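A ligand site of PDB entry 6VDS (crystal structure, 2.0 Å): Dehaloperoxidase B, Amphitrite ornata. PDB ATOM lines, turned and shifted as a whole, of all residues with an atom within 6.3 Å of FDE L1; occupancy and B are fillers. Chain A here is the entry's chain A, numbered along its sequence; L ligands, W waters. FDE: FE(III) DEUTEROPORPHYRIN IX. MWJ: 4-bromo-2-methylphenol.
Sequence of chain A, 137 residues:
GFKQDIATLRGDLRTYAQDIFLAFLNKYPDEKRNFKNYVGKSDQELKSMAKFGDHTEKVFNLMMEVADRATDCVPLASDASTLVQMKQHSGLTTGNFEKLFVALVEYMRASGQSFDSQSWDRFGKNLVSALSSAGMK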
ATOM      1  N   PHE A  21      16.840 -25.205   2.500  1.00  0.00           N
ATOM      2  CA  PHE A  21      16.959 -24.362   3.706  1.00  0.00           C
ATOM      3  C   PHE A  21      18.215 -23.530   3.557  1.00  0.00           C
ATOM      4  O   PHE A  21      18.138 -22.349   3.924  1.00  0.00           O
ATOM      5  CB  PHE A  21      16.929 -25.212   4.965  1.00  0.00           C
ATOM      6  CG  PHE A  21      16.502 -24.404   6.163  1.00  0.00           C
ATOM      7  CD1 PHE A  21      15.279 -23.769   6.152  1.00  0.00           C
ATOM      8  CD2 PHE A  21      17.336 -24.245   7.257  1.00  0.00           C
ATOM      9  CE1 PHE A  21      14.861 -23.024   7.244  1.00  0.00           C
ATOM     10  CE2 PHE A  21      16.901 -23.520   8.360  1.00  0.00           C
ATOM     11  CZ  PHE A  21      15.682 -22.895   8.336  1.00  0.00           C
ATOM     12  N   ASN A  34      18.080 -15.886  13.655  1.00  0.00           N
ATOM     13  CA  ASN A  34      16.983 -16.585  14.364  1.00  0.00           C
ATOM     14  C   ASN A  34      17.501 -17.934  14.883  1.00  0.00           C
ATOM     15  O   ASN A  34      16.866 -18.503  15.795  1.00  0.00           O
ATOM     16  CB  ASN A  34      15.751 -16.679  13.461  1.00  0.00           C
ATOM     17  CG  ASN A  34      15.230 -15.303  13.138  1.00  0.00           C
ATOM     18  OD1 ASN A  34      15.049 -14.478  14.043  1.00  0.00           O
ATOM     19  ND2 ASN A  34      15.045 -15.010  11.857  1.00  0.00           N
ATOM     20  N   PHE A  35      18.642 -18.381  14.332  1.00  0.00           N
ATOM     21  CA  PHE A  35      19.411 -19.619  14.667  1.00  0.00           C
ATOM     22  C   PHE A  35      20.886 -19.238  14.933  1.00  0.00           C
ATOM     23  O   PHE A  35      21.782 -19.843  14.334  1.00  0.00           O
ATOM     24  CB  PHE A  35      19.267 -20.612  13.495  1.00  0.00           C
ATOM     25  CG  PHE A  35      17.935 -20.644  12.760  1.00  0.00           C
ATOM     26  CD1 PHE A  35      17.680 -19.806  11.688  1.00  0.00           C
ATOM     27  CD2 PHE A  35      16.970 -21.571  13.093  1.00  0.00           C
ATOM     28  CE1 PHE A  35      16.477 -19.872  10.997  1.00  0.00           C
ATOM     29  CE2 PHE A  35      15.759 -21.658  12.408  1.00  0.00           C
ATOM     30  CZ  PHE A  35      15.523 -20.809  11.348  1.00  0.00           C
ATOM     31  N   LYS A  36      21.112 -18.242  15.805  1.00  0.00           N
ATOM     32  CA  LYS A  36      22.327 -17.381  15.989  1.00  0.00           C
ATOM     33  C   LYS A  36      23.684 -18.082  15.730  1.00  0.00           C
ATOM     34  O   LYS A  36      24.565 -17.446  15.124  1.00  0.00           O
ATOM     35  CB  LYS A  36      22.351 -16.833  17.425  1.00  0.00           C
ATOM     36  N   ASN A  37      23.865 -19.280  16.285  1.00  0.00           N
ATOM     37  CA  ASN A  37      24.998 -20.235  16.074  1.00  0.00           C
ATOM     38  C   ASN A  37      25.214 -20.598  14.595  1.00  0.00           C
ATOM     39  O   ASN A  37      26.230 -21.230  14.286  1.00  0.00           O
ATOM     40  CB  ASN A  37      24.704 -21.530  16.826  1.00  0.00           C
ATOM     41  CG  ASN A  37      23.297 -22.020  16.537  1.00  0.00           C
ATOM     42  OD1 ASN A  37      23.110 -23.029  15.852  1.00  0.00           O
ATOM     43  ND2 ASN A  37      22.311 -21.291  17.020  1.00  0.00           N
ATOM     44  N   LYS A  51      22.058 -30.066  15.207  1.00  0.00           N
ATOM     45  CA  LYS A  51      20.714 -29.439  15.347  1.00  0.00           C
ATOM     46  C   LYS A  51      20.258 -28.876  14.000  1.00  0.00           C
ATOM     47  O   LYS A  51      19.016 -28.798  13.786  1.00  0.00           O
ATOM     48  CB  LYS A  51      20.715 -28.343  16.412  1.00  0.00           C
ATOM     49  CG  LYS A  51      20.717 -28.846  17.855  1.00  0.00           C
ATOM     50  CD  LYS A  51      20.582 -27.745  18.882  1.00  0.00           C
ATOM     51  CE  LYS A  51      20.664 -28.257  20.303  1.00  0.00           C
ATOM     52  NZ  LYS A  51      20.969 -27.176  21.274  1.00  0.00           N
ATOM     53  N   HIS A  55      16.917 -30.386  12.956  1.00  0.00           N
ATOM     54  CA  HIS A  55      15.881 -29.324  12.956  1.00  0.00           C
ATOM     55  C   HIS A  55      15.359 -29.105  11.548  1.00  0.00           C
ATOM     56  O   HIS A  55      14.144 -28.993  11.420  1.00  0.00           O
ATOM     57  CB  HIS A  55      16.325 -28.000  13.571  1.00  0.00           C
ATOM     58  CG  HIS A  55      15.182 -27.065  13.765  1.00  0.00           C
ATOM     59  ND1 HIS A  55      14.902 -26.072  12.850  1.00  0.00           N
ATOM     60  CD2 HIS A  55      14.268 -26.959  14.745  1.00  0.00           C
ATOM     61  CE1 HIS A  55      13.872 -25.377  13.257  1.00  0.00           C
ATOM     62  NE2 HIS A  55      13.437 -25.902  14.420  1.00  0.00           N
ATOM     63  N   LYS A  58      13.036 -31.845  10.568  1.00  0.00           N
ATOM     64  CA  LYS A  58      11.737 -31.798  11.299  1.00  0.00           C
ATOM     65  C   LYS A  58      10.877 -30.670  10.722  1.00  0.00           C
ATOM     66  O   LYS A  58       9.686 -30.902  10.493  1.00  0.00           O
ATOM     67  CB  LYS A  58      11.992 -31.681  12.809  1.00  0.00           C
ATOM     68  CG  LYS A  58      12.467 -32.957  13.476  1.00  0.00           C
ATOM     69  CD  LYS A  58      12.555 -32.845  14.978  1.00  0.00           C
ATOM     70  CE  LYS A  58      13.378 -33.952  15.610  1.00  0.00           C
ATOM     71  NZ  LYS A  58      13.358 -33.875  17.083  1.00  0.00           N
ATOM     72  N   VAL A  59      11.471 -29.524  10.371  1.00  0.00           N
ATOM     73  CA  VAL A  59      10.734 -28.427   9.667  1.00  0.00           C
ATOM     74  C   VAL A  59       9.986 -29.017   8.475  1.00  0.00           C
ATOM     75  O   VAL A  59       8.771 -28.708   8.291  1.00  0.00           O
ATOM     76  CB  VAL A  59      11.654 -27.285   9.199  1.00  0.00           C
ATOM     77  CG1 VAL A  59      10.866 -26.304   8.345  1.00  0.00           C
ATOM     78  CG2 VAL A  59      12.317 -26.566  10.387  1.00  0.00           C
ATOM     79  N   LEU A  62       7.351 -31.856   9.040  1.00  0.00           N
ATOM     80  CA  LEU A  62       6.094 -31.121   9.333  1.00  0.00           C
ATOM     81  C   LEU A  62       5.511 -30.469   8.066  1.00  0.00           C
ATOM     82  O   LEU A  62       4.327 -30.641   7.808  1.00  0.00           O
ATOM     83  CB  LEU A  62       6.338 -30.059  10.399  1.00  0.00           C
ATOM     84  N   MET A  63       6.289 -29.711   7.306  1.00  0.00           N
ATOM     85  CA  MET A  63       5.694 -28.995   6.159  1.00  0.00           C
ATOM     86  C   MET A  63       5.185 -30.014   5.116  1.00  0.00           C
ATOM     87  O   MET A  63       4.186 -29.713   4.485  1.00  0.00           O
ATOM     88  CB  MET A  63       6.651 -27.988   5.514  1.00  0.00           C
ATOM     89  CG  MET A  63       5.957 -26.689   5.110  1.00  0.00           C
ATOM     90  SD  MET A  63       6.193 -25.352   6.306  1.00  0.00           S
ATOM     91  CE  MET A  63       5.343 -25.990   7.747  1.00  0.00           C
ATOM     92  N   LEU A  83       0.302 -24.853  14.413  1.00  0.00           N
ATOM     93  CA  LEU A  83       1.620 -24.236  14.088  1.00  0.00           C
ATOM     94  C   LEU A  83       1.806 -22.944  14.876  1.00  0.00           C
ATOM     95  O   LEU A  83       2.939 -22.695  15.367  1.00  0.00           O
ATOM     96  CB  LEU A  83       1.709 -23.953  12.581  1.00  0.00           C
ATOM     97  CG  LEU A  83       2.228 -25.097  11.717  1.00  0.00           C
ATOM     98  CD1 LEU A  83       1.824 -24.906  10.254  1.00  0.00           C
ATOM     99  CD2 LEU A  83       3.736 -25.250  11.851  1.00  0.00           C
ATOM    100  N   MET A  86       2.321 -24.012  18.487  1.00  0.00           N
ATOM    101  CA  MET A  86       3.559 -24.831  18.682  1.00  0.00           C
ATOM    102  C   MET A  86       4.402 -24.308  19.858  1.00  0.00           C
ATOM    103  O   MET A  86       4.856 -23.136  19.805  1.00  0.00           O
ATOM    104  CB  MET A  86       4.404 -24.839  17.402  1.00  0.00           C
ATOM    105  CG  MET A  86       5.570 -25.826  17.428  1.00  0.00           C
ATOM    106  SD  MET A  86       6.347 -26.088  15.784  1.00  0.00           S
ATOM    107  CE  MET A  86       5.002 -26.915  14.934  1.00  0.00           C
ATOM    108  N   LYS A  87       4.578 -25.110  20.915  1.00  0.00           N
ATOM    109  CA  LYS A  87       5.482 -24.786  22.054  1.00  0.00           C
ATOM    110  C   LYS A  87       6.860 -24.426  21.488  1.00  0.00           C
ATOM    111  O   LYS A  87       7.286 -25.067  20.491  1.00  0.00           O
ATOM    112  CB  LYS A  87       5.619 -25.952  23.036  1.00  0.00           C
ATOM    113  N   GLN A  88       7.513 -23.427  22.080  1.00  0.00           N
ATOM    114  CA  GLN A  88       8.909 -23.017  21.767  1.00  0.00           C
ATOM    115  C   GLN A  88       8.974 -22.339  20.404  1.00  0.00           C
ATOM    116  O   GLN A  88      10.101 -22.194  19.878  1.00  0.00           O
ATOM    117  CB  GLN A  88       9.879 -24.210  21.789  1.00  0.00           C
ATOM    118  CG  GLN A  88       9.889 -25.008  23.079  1.00  0.00           C
ATOM    119  CD  GLN A  88      11.204 -25.704  23.329  1.00  0.00           C
ATOM    120  OE1 GLN A  88      12.266 -25.172  23.040  1.00  0.00           O
ATOM    121  NE2 GLN A  88      11.144 -26.887  23.929  1.00  0.00           N
ATOM    122  N   HIS A  89       7.841 -21.899  19.844  1.00  0.00           N
ATOM    123  CA  HIS A  89       7.809 -21.264  18.493  1.00  0.00           C
ATOM    124  C   HIS A  89       6.907 -20.018  18.488  1.00  0.00           C
ATOM    125  O   HIS A  89       6.593 -19.553  17.387  1.00  0.00           O
ATOM    126  CB  HIS A  89       7.408 -22.301  17.435  1.00  0.00           C
ATOM    127  CG  HIS A  89       8.460 -23.338  17.241  1.00  0.00           C
ATOM    128  ND1 HIS A  89       8.619 -24.386  18.124  1.00  0.00           N
ATOM    129  CD2 HIS A  89       9.399 -23.493  16.283  1.00  0.00           C
ATOM    130  CE1 HIS A  89       9.601 -25.152  17.713  1.00  0.00           C
ATOM    131  NE2 HIS A  89      10.110 -24.614  16.599  1.00  0.00           N
ATOM    132  N   LEU A  92       7.707 -17.214  15.711  1.00  0.00           N
ATOM    133  CA  LEU A  92       7.685 -17.394  14.221  1.00  0.00           C
ATOM    134  C   LEU A  92       6.908 -16.236  13.571  1.00  0.00           C
ATOM    135  O   LEU A  92       6.000 -15.709  14.227  1.00  0.00           O
ATOM    136  CB  LEU A  92       7.028 -18.735  13.879  1.00  0.00           C
ATOM    137  CG  LEU A  92       7.748 -19.989  14.369  1.00  0.00           C
ATOM    138  CD1 LEU A  92       6.983 -21.228  13.900  1.00  0.00           C
ATOM    139  CD2 LEU A  92       9.187 -20.035  13.881  1.00  0.00           C
ATOM    140  N   PHE A  97       8.198 -17.138   6.622  1.00  0.00           N
ATOM    141  CA  PHE A  97       7.653 -18.261   5.813  1.00  0.00           C
ATOM    142  C   PHE A  97       7.646 -17.879   4.321  1.00  0.00           C
ATOM    143  O   PHE A  97       8.106 -18.703   3.521  1.00  0.00           O
ATOM    144  CB  PHE A  97       6.283 -18.723   6.332  1.00  0.00           C
ATOM    145  CG  PHE A  97       6.358 -19.704   7.491  1.00  0.00           C
ATOM    146  CD1 PHE A  97       6.658 -21.034   7.269  1.00  0.00           C
ATOM    147  CD2 PHE A  97       6.130 -19.277   8.789  1.00  0.00           C
ATOM    148  CE1 PHE A  97       6.694 -21.939   8.320  1.00  0.00           C
ATOM    149  CE2 PHE A  97       6.166 -20.183   9.840  1.00  0.00           C
ATOM    150  CZ  PHE A  97       6.447 -21.504   9.605  1.00  0.00           C
ATOM    151  N   LEU A 100      10.969 -18.336   3.073  1.00  0.00           N
ATOM    152  CA  LEU A 100      11.270 -19.765   2.890  1.00  0.00           C
ATOM    153  C   LEU A 100      10.697 -20.196   1.543  1.00  0.00           C
ATOM    154  O   LEU A 100      11.422 -20.831   0.766  1.00  0.00           O
ATOM    155  CB  LEU A 100      10.718 -20.624   4.044  1.00  0.00           C
ATOM    156  CG  LEU A 100      10.976 -22.132   3.924  1.00  0.00           C
ATOM    157  CD1 LEU A 100      12.461 -22.492   3.875  1.00  0.00           C
ATOM    158  CD2 LEU A 100      10.314 -22.873   5.090  1.00  0.00           C
HETATM  159  CHA FDE L   1      13.527 -23.759  17.725  1.00  0.00           C
HETATM  160  C1A FDE L   1      13.216 -25.174  17.903  1.00  0.00           C
HETATM  161  C2A FDE L   1      13.738 -25.992  19.040  1.00  0.00           C
HETATM  162  CAA FDE L   1      14.703 -25.569  20.127  1.00  0.00           C
HETATM  163  CBA FDE L   1      16.047 -25.211  19.501  1.00  0.00           C
HETATM  164  CGA FDE L   1      17.140 -26.234  19.720  1.00  0.00           C
HETATM  165  O1A FDE L   1      16.902 -27.458  19.547  1.00  0.00           O
HETATM  166  O2A FDE L   1      18.265 -25.800  20.081  1.00  0.00           O
HETATM  167  C3A FDE L   1      13.172 -27.356  18.855  1.00  0.00           C
HETATM  168  CMA FDE L   1      13.455 -28.550  19.731  1.00  0.00           C
HETATM  169  C4A FDE L   1      12.335 -27.281  17.600  1.00  0.00           C
HETATM  170  NA  FDE L   1      12.230 -25.888  17.119  1.00  0.00           N
HETATM  171  CHB FDE L   1      11.532 -28.392  17.065  1.00  0.00           C
HETATM  172  C1B FDE L   1      10.653 -28.265  15.878  1.00  0.00           C
HETATM  173  C2B FDE L   1       9.847 -29.340  15.540  1.00  0.00           C
HETATM  174  C3B FDE L   1       9.166 -28.885  14.442  1.00  0.00           C
HETATM  175  CME FDE L   1       8.176 -29.816  13.786  1.00  0.00           C
HETATM  176  C4B FDE L   1       9.623 -27.498  14.216  1.00  0.00           C
HETATM  177  NB  FDE L   1      10.553 -27.152  15.120  1.00  0.00           N
HETATM  178  CHC FDE L   1       9.165 -26.626  13.132  1.00  0.00           C
HETATM  179  C1C FDE L   1       9.732 -25.308  12.835  1.00  0.00           C
HETATM  180  C2C FDE L   1       9.277 -24.678  11.692  1.00  0.00           C
HETATM  181  C3C FDE L   1      10.004 -23.516  11.691  1.00  0.00           C
HETATM  182  CMF FDE L   1       9.748 -22.580  10.558  1.00  0.00           C
HETATM  183  C4C FDE L   1      10.880 -23.553  12.875  1.00  0.00           C
HETATM  184  NC  FDE L   1      10.680 -24.687  13.553  1.00  0.00           N
HETATM  185  CHD FDE L   1      11.821 -22.492  13.287  1.00  0.00           C
HETATM  186  C1D FDE L   1      12.535 -22.449  14.572  1.00  0.00           C
HETATM  187  C2D FDE L   1      13.303 -21.242  15.007  1.00  0.00           C
HETATM  188  CMD FDE L   1      13.532 -19.948  14.282  1.00  0.00           C
HETATM  189  C3D FDE L   1      13.802 -21.625  16.332  1.00  0.00           C
HETATM  190  CAD FDE L   1      14.656 -20.829  17.291  1.00  0.00           C
HETATM  191  CBD FDE L   1      16.042 -21.444  17.485  1.00  0.00           C
HETATM  192  CGD FDE L   1      16.706 -20.923  18.751  1.00  0.00           C
HETATM  193  O1D FDE L   1      17.937 -20.749  18.729  1.00  0.00           O
HETATM  194  O2D FDE L   1      16.019 -20.679  19.768  1.00  0.00           O
HETATM  195  C4D FDE L   1      13.248 -22.986  16.509  1.00  0.00           C
HETATM  196  ND  FDE L   1      12.519 -23.461  15.473  1.00  0.00           N
HETATM  197 FE   FDE L   1      11.569 -25.335  15.313  1.00  0.00          FE
HETATM  198  C4  MWJ L   2       9.495 -18.517  10.446  1.00  0.00           C
HETATM  199  C1  MWJ L   2      12.857 -17.474  11.882  1.00  0.00           C
HETATM  200  C7  MWJ L   2      12.164 -19.201  10.183  1.00  0.00           C
HETATM  201  C2  MWJ L   2      11.804 -18.191  11.079  1.00  0.00           C
HETATM  202  C6  MWJ L   2      11.188 -19.843   9.436  1.00  0.00           C
HETATM  203  C3  MWJ L   2      10.453 -17.854  11.202  1.00  0.00           C
HETATM  204  C5  MWJ L   2       9.860 -19.507   9.558  1.00  0.00           C
HETATM  205 BR1  MWJ L   2      11.698 -21.230   8.231  1.00  0.00          BR
HETATM  206  O1  MWJ L   2      10.074 -16.866  12.064  1.00  0.00           O
HETATM  207  O   HOH W   1      17.008 -26.134  16.480  1.00  0.00           O
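Residues that only touch FDE L1: Asn 34, Phe 35, Lys 58, Val 59, Leu 62, Met 86, Gln 88, Leu 92 and Phe 97.
12 residues have an atom within 4 Å of FDE L1: Asn 34, Phe 35, Lys 51, His 55, Lys 58, Val 59, Leu 62, Met 86, Gln 88, His 89, Leu 92 and Phe 97.
An iron atom (FE) of FDE L1 is bound by a ring nitrogen (NE2) of His 89, at 2.1 Å.
FE of FDE L1 is bound by NE2 of His 55, at 2.1 Å.
O2A of FDE L1 lies within salt-bridge range of NZ of Lys 51, at 3.3 Å.
The side-chain sulfur (SD) of Met 86 sits close to a ring nitrogen (ND1) of His 89, 3.7 Å away.
ND1 of His 89 lies within hydrogen-bond range of O of Lys 87, at 2.8 Å.
O of Phe 35 sits at hydrogen-bond distance from ND2 of Asn 37, at 3.1 Å.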
